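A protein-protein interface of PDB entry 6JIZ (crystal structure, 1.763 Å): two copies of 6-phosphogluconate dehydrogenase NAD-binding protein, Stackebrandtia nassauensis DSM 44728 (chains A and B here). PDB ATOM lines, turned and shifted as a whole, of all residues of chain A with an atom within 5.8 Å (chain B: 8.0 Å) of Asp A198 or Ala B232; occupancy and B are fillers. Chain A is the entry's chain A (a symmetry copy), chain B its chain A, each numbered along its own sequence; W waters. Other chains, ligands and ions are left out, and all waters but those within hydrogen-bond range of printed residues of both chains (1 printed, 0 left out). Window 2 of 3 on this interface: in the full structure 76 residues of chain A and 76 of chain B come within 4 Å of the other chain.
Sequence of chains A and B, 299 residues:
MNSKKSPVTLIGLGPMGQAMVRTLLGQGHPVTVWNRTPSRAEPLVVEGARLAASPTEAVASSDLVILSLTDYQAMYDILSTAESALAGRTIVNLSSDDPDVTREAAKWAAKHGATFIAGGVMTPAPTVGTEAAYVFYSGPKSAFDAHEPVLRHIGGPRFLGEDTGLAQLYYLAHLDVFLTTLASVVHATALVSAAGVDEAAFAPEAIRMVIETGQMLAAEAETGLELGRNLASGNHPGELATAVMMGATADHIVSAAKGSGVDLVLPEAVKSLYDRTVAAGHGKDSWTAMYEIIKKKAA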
ATOM      1  N   SER A 193      27.102  13.586  30.949  1.00  0.00           N
ATOM      2  CA  SER A 193      26.605  14.948  30.820  1.00  0.00           C
ATOM      3  C   SER A 193      26.308  15.595  32.165  1.00  0.00           C
ATOM      4  O   SER A 193      26.296  16.834  32.244  1.00  0.00           O
ATOM      5  CB  SER A 193      25.364  14.975  29.933  1.00  0.00           C
ATOM      6  OG  SER A 193      25.769  14.706  28.598  1.00  0.00           O
ATOM      7  N   GLY A 196      28.618  18.227  32.964  1.00  0.00           N
ATOM      8  CA  GLY A 196      28.666  19.403  32.114  1.00  0.00           C
ATOM      9  C   GLY A 196      29.081  19.141  30.683  1.00  0.00           C
ATOM     10  O   GLY A 196      29.085  20.078  29.875  1.00  0.00           O
ATOM     11  N   VAL A 197      29.408  17.893  30.342  1.00  0.00           N
ATOM     12  CA  VAL A 197      29.805  17.544  28.985  1.00  0.00           C
ATOM     13  C   VAL A 197      28.584  17.621  28.075  1.00  0.00           C
ATOM     14  O   VAL A 197      27.483  17.209  28.461  1.00  0.00           O
ATOM     15  CB  VAL A 197      30.432  16.134  28.978  1.00  0.00           C
ATOM     16  CG1 VAL A 197      30.661  15.622  27.556  1.00  0.00           C
ATOM     17  CG2 VAL A 197      31.756  16.121  29.768  1.00  0.00           C
ATOM     18  N   ASP A 198      28.774  18.187  26.879  1.00  0.00           N
ATOM     19  CA  ASP A 198      27.737  18.266  25.839  1.00  0.00           C
ATOM     20  C   ASP A 198      27.254  16.862  25.456  1.00  0.00           C
ATOM     21  O   ASP A 198      28.060  16.005  25.087  1.00  0.00           O
ATOM     22  CB  ASP A 198      28.342  18.993  24.633  1.00  0.00           C
ATOM     23  CG  ASP A 198      27.374  19.199  23.450  1.00  0.00           C
ATOM     24  OD1 ASP A 198      26.168  18.863  23.494  1.00  0.00           O
ATOM     25  OD2 ASP A 198      27.878  19.732  22.438  1.00  0.00           O
ATOM     26  N   GLU A 199      25.938  16.617  25.567  1.00  0.00           N
ATOM     27  CA  GLU A 199      25.391  15.304  25.201  1.00  0.00           C
ATOM     28  C   GLU A 199      25.813  14.895  23.798  1.00  0.00           C
ATOM     29  O   GLU A 199      26.078  13.712  23.536  1.00  0.00           O
ATOM     30  CB  GLU A 199      23.859  15.308  25.296  1.00  0.00           C
ATOM     31  CG  GLU A 199      23.306  15.341  26.693  1.00  0.00           C
ATOM     32  CD  GLU A 199      23.120  16.751  27.229  1.00  0.00           C
ATOM     33  OE1 GLU A 199      23.638  17.705  26.612  1.00  0.00           O
ATOM     34  OE2 GLU A 199      22.456  16.899  28.274  1.00  0.00           O
ATOM     35  N   ALA A 200      25.884  15.862  22.878  1.00  0.00           N
ATOM     36  CA  ALA A 200      26.260  15.571  21.501  1.00  0.00           C
ATOM     37  C   ALA A 200      27.705  15.122  21.375  1.00  0.00           C
ATOM     38  O   ALA A 200      28.056  14.484  20.377  1.00  0.00           O
ATOM     39  CB  ALA A 200      26.020  16.796  20.617  1.00  0.00           C
ATOM     40  N   ALA A 201      28.552  15.436  22.363  1.00  0.00           N
ATOM     41  CA  ALA A 201      29.932  14.975  22.326  1.00  0.00           C
ATOM     42  C   ALA A 201      30.044  13.504  22.725  1.00  0.00           C
ATOM     43  O   ALA A 201      30.867  12.768  22.171  1.00  0.00           O
ATOM     44  CB  ALA A 201      30.793  15.841  23.253  1.00  0.00           C
ATOM     45  N   PHE A 202      29.254  13.065  23.699  1.00  0.00           N
ATOM     46  CA  PHE A 202      29.439  11.716  24.218  1.00  0.00           C
ATOM     47  C   PHE A 202      28.516  10.677  23.591  1.00  0.00           C
ATOM     48  O   PHE A 202      28.921   9.515  23.467  1.00  0.00           O
ATOM     49  CB  PHE A 202      29.257  11.669  25.741  1.00  0.00           C
ATOM     50  CG  PHE A 202      29.632  10.332  26.332  1.00  0.00           C
ATOM     51  CD1 PHE A 202      30.962  10.021  26.568  1.00  0.00           C
ATOM     52  CD2 PHE A 202      28.660   9.371  26.598  1.00  0.00           C
ATOM     53  CE1 PHE A 202      31.323   8.772  27.079  1.00  0.00           C
ATOM     54  CE2 PHE A 202      29.014   8.132  27.105  1.00  0.00           C
ATOM     55  CZ  PHE A 202      30.351   7.831  27.332  1.00  0.00           C
ATOM     56  N   ALA A 203      27.289  11.038  23.214  1.00  0.00           N
ATOM     57  CA  ALA A 203      26.383  10.035  22.647  1.00  0.00           C
ATOM     58  C   ALA A 203      27.008   9.231  21.507  1.00  0.00           C
ATOM     59  O   ALA A 203      26.819   8.002  21.489  1.00  0.00           O
ATOM     60  CB  ALA A 203      25.075  10.696  22.178  1.00  0.00           C
ATOM     61  N   TYR B 170      34.297   8.846  31.999  1.00  0.00           N
ATOM     62  CA  TYR B 170      34.091   8.347  30.639  1.00  0.00           C
ATOM     63  C   TYR B 170      34.277   6.836  30.582  1.00  0.00           C
ATOM     64  O   TYR B 170      33.516   6.133  29.904  1.00  0.00           O
ATOM     65  CB  TYR B 170      35.059   9.012  29.658  1.00  0.00           C
ATOM     66  CG  TYR B 170      34.709  10.420  29.165  1.00  0.00           C
ATOM     67  CD1 TYR B 170      34.488  11.468  30.054  1.00  0.00           C
ATOM     68  CD2 TYR B 170      34.661  10.691  27.805  1.00  0.00           C
ATOM     69  CE1 TYR B 170      34.219  12.767  29.592  1.00  0.00           C
ATOM     70  CE2 TYR B 170      34.384  11.969  27.331  1.00  0.00           C
ATOM     71  CZ  TYR B 170      34.168  13.000  28.231  1.00  0.00           C
ATOM     72  OH  TYR B 170      33.918  14.269  27.769  1.00  0.00           O
ATOM     73  N   GLU B 226      18.654  10.348  15.318  1.00  0.00           N
ATOM     74  CA  GLU B 226      19.830  11.132  15.689  1.00  0.00           C
ATOM     75  C   GLU B 226      19.824  11.246  17.213  1.00  0.00           C
ATOM     76  O   GLU B 226      19.318  12.211  17.783  1.00  0.00           O
ATOM     77  CB  GLU B 226      19.807  12.510  15.024  1.00  0.00           C
ATOM     78  CG  GLU B 226      19.374  12.508  13.574  1.00  0.00           C
ATOM     79  CD  GLU B 226      18.765  13.838  13.161  1.00  0.00           C
ATOM     80  OE1 GLU B 226      17.565  14.064  13.444  1.00  0.00           O
ATOM     81  OE2 GLU B 226      19.493  14.661  12.567  1.00  0.00           O
ATOM     82  N   LEU B 227      20.384  10.231  17.874  1.00  0.00           N
ATOM     83  CA  LEU B 227      20.264  10.136  19.326  1.00  0.00           C
ATOM     84  C   LEU B 227      20.898  11.338  20.020  1.00  0.00           C
ATOM     85  O   LEU B 227      20.277  11.975  20.884  1.00  0.00           O
ATOM     86  CB  LEU B 227      20.904   8.835  19.805  1.00  0.00           C
ATOM     87  CG  LEU B 227      20.920   8.605  21.311  1.00  0.00           C
ATOM     88  CD1 LEU B 227      19.552   8.843  21.887  1.00  0.00           C
ATOM     89  CD2 LEU B 227      21.331   7.183  21.564  1.00  0.00           C
ATOM     90  N   GLY B 228      22.138  11.662  19.655  1.00  0.00           N
ATOM     91  CA  GLY B 228      22.820  12.772  20.298  1.00  0.00           C
ATOM     92  C   GLY B 228      22.102  14.087  20.092  1.00  0.00           C
ATOM     93  O   GLY B 228      22.089  14.939  20.985  1.00  0.00           O
ATOM     94  N   ARG B 229      21.476  14.257  18.926  1.00  0.00           N
ATOM     95  CA  ARG B 229      20.692  15.460  18.665  1.00  0.00           C
ATOM     96  C   ARG B 229      19.503  15.566  19.613  1.00  0.00           C
ATOM     97  O   ARG B 229      19.250  16.637  20.179  1.00  0.00           O
ATOM     98  CB  ARG B 229      20.231  15.460  17.208  1.00  0.00           C
ATOM     99  CG  ARG B 229      19.487  16.715  16.803  1.00  0.00           C
ATOM    100  CD  ARG B 229      19.215  16.743  15.306  1.00  0.00           C
ATOM    101  NE  ARG B 229      18.521  17.969  14.923  1.00  0.00           N
ATOM    102  CZ  ARG B 229      18.165  18.266  13.676  1.00  0.00           C
ATOM    103  NH1 ARG B 229      18.440  17.423  12.688  1.00  0.00           N
ATOM    104  NH2 ARG B 229      17.534  19.405  13.422  1.00  0.00           N
ATOM    105  N   ASN B 230      18.757  14.471  19.798  1.00  0.00           N
ATOM    106  CA  ASN B 230      17.636  14.484  20.738  1.00  0.00           C
ATOM    107  C   ASN B 230      18.099  14.852  22.145  1.00  0.00           C
ATOM    108  O   ASN B 230      17.511  15.721  22.800  1.00  0.00           O
ATOM    109  CB  ASN B 230      16.942  13.117  20.761  1.00  0.00           C
ATOM    110  CG  ASN B 230      16.070  12.866  19.532  1.00  0.00           C
ATOM    111  OD1 ASN B 230      16.242  13.499  18.492  1.00  0.00           O
ATOM    112  ND2 ASN B 230      15.129  11.923  19.653  1.00  0.00           N
ATOM    113  N   LEU B 231      19.146  14.178  22.639  1.00  0.00           N
ATOM    114  CA  LEU B 231      19.570  14.403  24.019  1.00  0.00           C
ATOM    115  C   LEU B 231      20.149  15.800  24.205  1.00  0.00           C
ATOM    116  O   LEU B 231      19.921  16.432  25.240  1.00  0.00           O
ATOM    117  CB  LEU B 231      20.597  13.353  24.448  1.00  0.00           C
ATOM    118  CG  LEU B 231      20.256  11.878  24.218  1.00  0.00           C
ATOM    119  CD1 LEU B 231      21.296  10.969  24.894  1.00  0.00           C
ATOM    120  CD2 LEU B 231      18.856  11.560  24.711  1.00  0.00           C
ATOM    121  N   ALA B 232      20.907  16.294  23.222  1.00  0.00           N
ATOM    122  CA  ALA B 232      21.537  17.606  23.376  1.00  0.00           C
ATOM    123  C   ALA B 232      20.516  18.735  23.271  1.00  0.00           C
ATOM    124  O   ALA B 232      20.616  19.743  23.986  1.00  0.00           O
ATOM    125  CB  ALA B 232      22.658  17.769  22.347  1.00  0.00           C
ATOM    126  N   SER B 233      19.496  18.564  22.426  1.00  0.00           N
ATOM    127  CA  SER B 233      18.526  19.630  22.210  1.00  0.00           C
ATOM    128  C   SER B 233      17.380  19.598  23.208  1.00  0.00           C
ATOM    129  O   SER B 233      16.710  20.619  23.386  1.00  0.00           O
ATOM    130  CB  SER B 233      17.955  19.546  20.793  1.00  0.00           C
ATOM    131  OG  SER B 233      17.120  18.405  20.675  1.00  0.00           O
ATOM    132  N   GLY B 234      17.139  18.461  23.862  1.00  0.00           N
ATOM    133  CA  GLY B 234      15.957  18.313  24.683  1.00  0.00           C
ATOM    134  C   GLY B 234      14.675  18.116  23.905  1.00  0.00           C
ATOM    135  O   GLY B 234      13.593  18.139  24.500  1.00  0.00           O
ATOM    136  N   ASN B 235      14.756  17.923  22.598  1.00  0.00           N
ATOM    137  CA  ASN B 235      13.585  17.659  21.771  1.00  0.00           C
ATOM    138  C   ASN B 235      13.594  16.187  21.391  1.00  0.00           C
ATOM    139  O   ASN B 235      14.557  15.706  20.780  1.00  0.00           O
ATOM    140  CB  ASN B 235      13.579  18.534  20.518  1.00  0.00           C
ATOM    141  CG  ASN B 235      13.493  20.015  20.839  1.00  0.00           C
ATOM    142  OD1 ASN B 235      12.938  20.411  21.871  1.00  0.00           O
ATOM    143  ND2 ASN B 235      14.038  20.846  19.950  1.00  0.00           N
ATOM    144  N   HIS B 236      12.510  15.483  21.720  1.00  0.00           N
ATOM    145  CA  HIS B 236      12.412  14.042  21.504  1.00  0.00           C
ATOM    146  C   HIS B 236      11.227  13.748  20.584  1.00  0.00           C
ATOM    147  O   HIS B 236      10.206  13.214  21.032  1.00  0.00           O
ATOM    148  CB  HIS B 236      12.269  13.316  22.840  1.00  0.00           C
ATOM    149  CG  HIS B 236      13.341  13.669  23.828  1.00  0.00           C
ATOM    150  ND1 HIS B 236      14.609  13.129  23.769  1.00  0.00           N
ATOM    151  CD2 HIS B 236      13.342  14.523  24.879  1.00  0.00           C
ATOM    152  CE1 HIS B 236      15.342  13.629  24.751  1.00  0.00           C
ATOM    153  NE2 HIS B 236      14.598  14.476  25.439  1.00  0.00           N
ATOM    154  N   TYR B 291      15.614  10.117  28.762  1.00  0.00           N
ATOM    155  CA  TYR B 291      16.735  10.936  29.207  1.00  0.00           C
ATOM    156  C   TYR B 291      16.289  11.991  30.210  1.00  0.00           C
ATOM    157  O   TYR B 291      17.015  12.299  31.163  1.00  0.00           O
ATOM    158  CB  TYR B 291      17.393  11.592  27.999  1.00  0.00           C
ATOM    159  CG  TYR B 291      18.598  12.422  28.381  1.00  0.00           C
ATOM    160  CD1 TYR B 291      19.774  11.807  28.804  1.00  0.00           C
ATOM    161  CD2 TYR B 291      18.561  13.809  28.329  1.00  0.00           C
ATOM    162  CE1 TYR B 291      20.892  12.562  29.165  1.00  0.00           C
ATOM    163  CE2 TYR B 291      19.682  14.572  28.682  1.00  0.00           C
ATOM    164  CZ  TYR B 291      20.842  13.939  29.107  1.00  0.00           C
ATOM    165  OH  TYR B 291      21.963  14.672  29.470  1.00  0.00           O
ATOM    166  N   GLU B 292      15.088  12.551  30.025  1.00  0.00           N
ATOM    167  CA  GLU B 292      14.618  13.584  30.941  1.00  0.00           C
ATOM    168  C   GLU B 292      14.293  13.023  32.326  1.00  0.00           C
ATOM    169  O   GLU B 292      14.328  13.777  33.308  1.00  0.00           O
ATOM    170  CB  GLU B 292      13.409  14.307  30.328  1.00  0.00           C
ATOM    171  CG  GLU B 292      13.640  14.784  28.888  1.00  0.00           C
ATOM    172  CD  GLU B 292      14.795  15.784  28.752  1.00  0.00           C
ATOM    173  OE1 GLU B 292      15.033  16.556  29.700  1.00  0.00           O
ATOM    174  OE2 GLU B 292      15.474  15.799  27.700  1.00  0.00           O
HETATM  175  O   HOH W   1      22.396  20.180  25.889  1.00  0.00           O
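Among the printed residues, merely in contact across the chains: Ser A193 with Tyr B291 (3.4 Å), Val A197 with Tyr B170 (3.5 Å), Asp A198 with Ala B232 (3.9 Å), Glu A199 with Leu B231 (3.8 Å), Glu A199 with Ala B232 (3.7 Å), Ala A200 with Ala B232 (3.8 Å), Phe A202 with Tyr B170 (3.9 Å) and Ala A203 with Gly B228 (3.6 Å).
No position is printed for both chains. Of the 9 pairs that touch across the chains among the printed residues, none has its exchanged pair printed and touching as well.
Of the 14 printed residues of chain B, 5 touch a printed residue of chain A. Hydrophobic or aromatic side chains of chain B that line the printed part of chain A: Tyr B170, Leu B231, Ala B232 and Tyr B291. Of the 9 printed residues of chain A, 7 touch a printed residue of chain B. Among the printed residues, no Asp or Glu carboxylate lies within 4 Å of a Lys or Arg side-chain nitrogen of the other chain.
Printed residues of chain B within 4 Å of Asp A198: Ala B232 (3.9 Å). Of the printed residues of chain B, Glu A199 touches Leu B231, Ala B232 and Tyr B291. Printed residues of chain B within 4 Å of Phe A202: Tyr B170. Printed residues of chain B within 4 Å of Ala A203: Gly B228 (3.6 Å). Printed residues of chain A within 4 Å of Gly B228: Ala A203. Printed residues of chain A within 4 Å of Ala B232: Asp A198, Glu A199 and Ala A200. Gly B234 touches none of the printed residues of chain A. His B236 touches none of the printed residues of chain A. Of the printed residues of chain A, Tyr B291 touches Ser A193 (3.4 Å) and Glu A199 (2.6 Å). The nearest printed residue of chain A that does not touch Ala B232 is Ala A201 (6.3 Å).
O of Val A197 sits at hydrogen-bond distance from OG of Ser A193 (3.0 Å). The side-chain carboxylate (OD1) of Asp A198 lies within hydrogen-bond range of the backbone NH (N) of Ala A200 (3.1 Å).
Water W1 bridges the backbone carbonyl oxygen (O) of Ala B232 (2.6 Å) and the side-chain carboxylate (OE1) of Glu A199 (2.9 Å).
OH of Tyr B291 is in hydrogen-bond range of OE2 of Glu A199 (2.6 Å).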
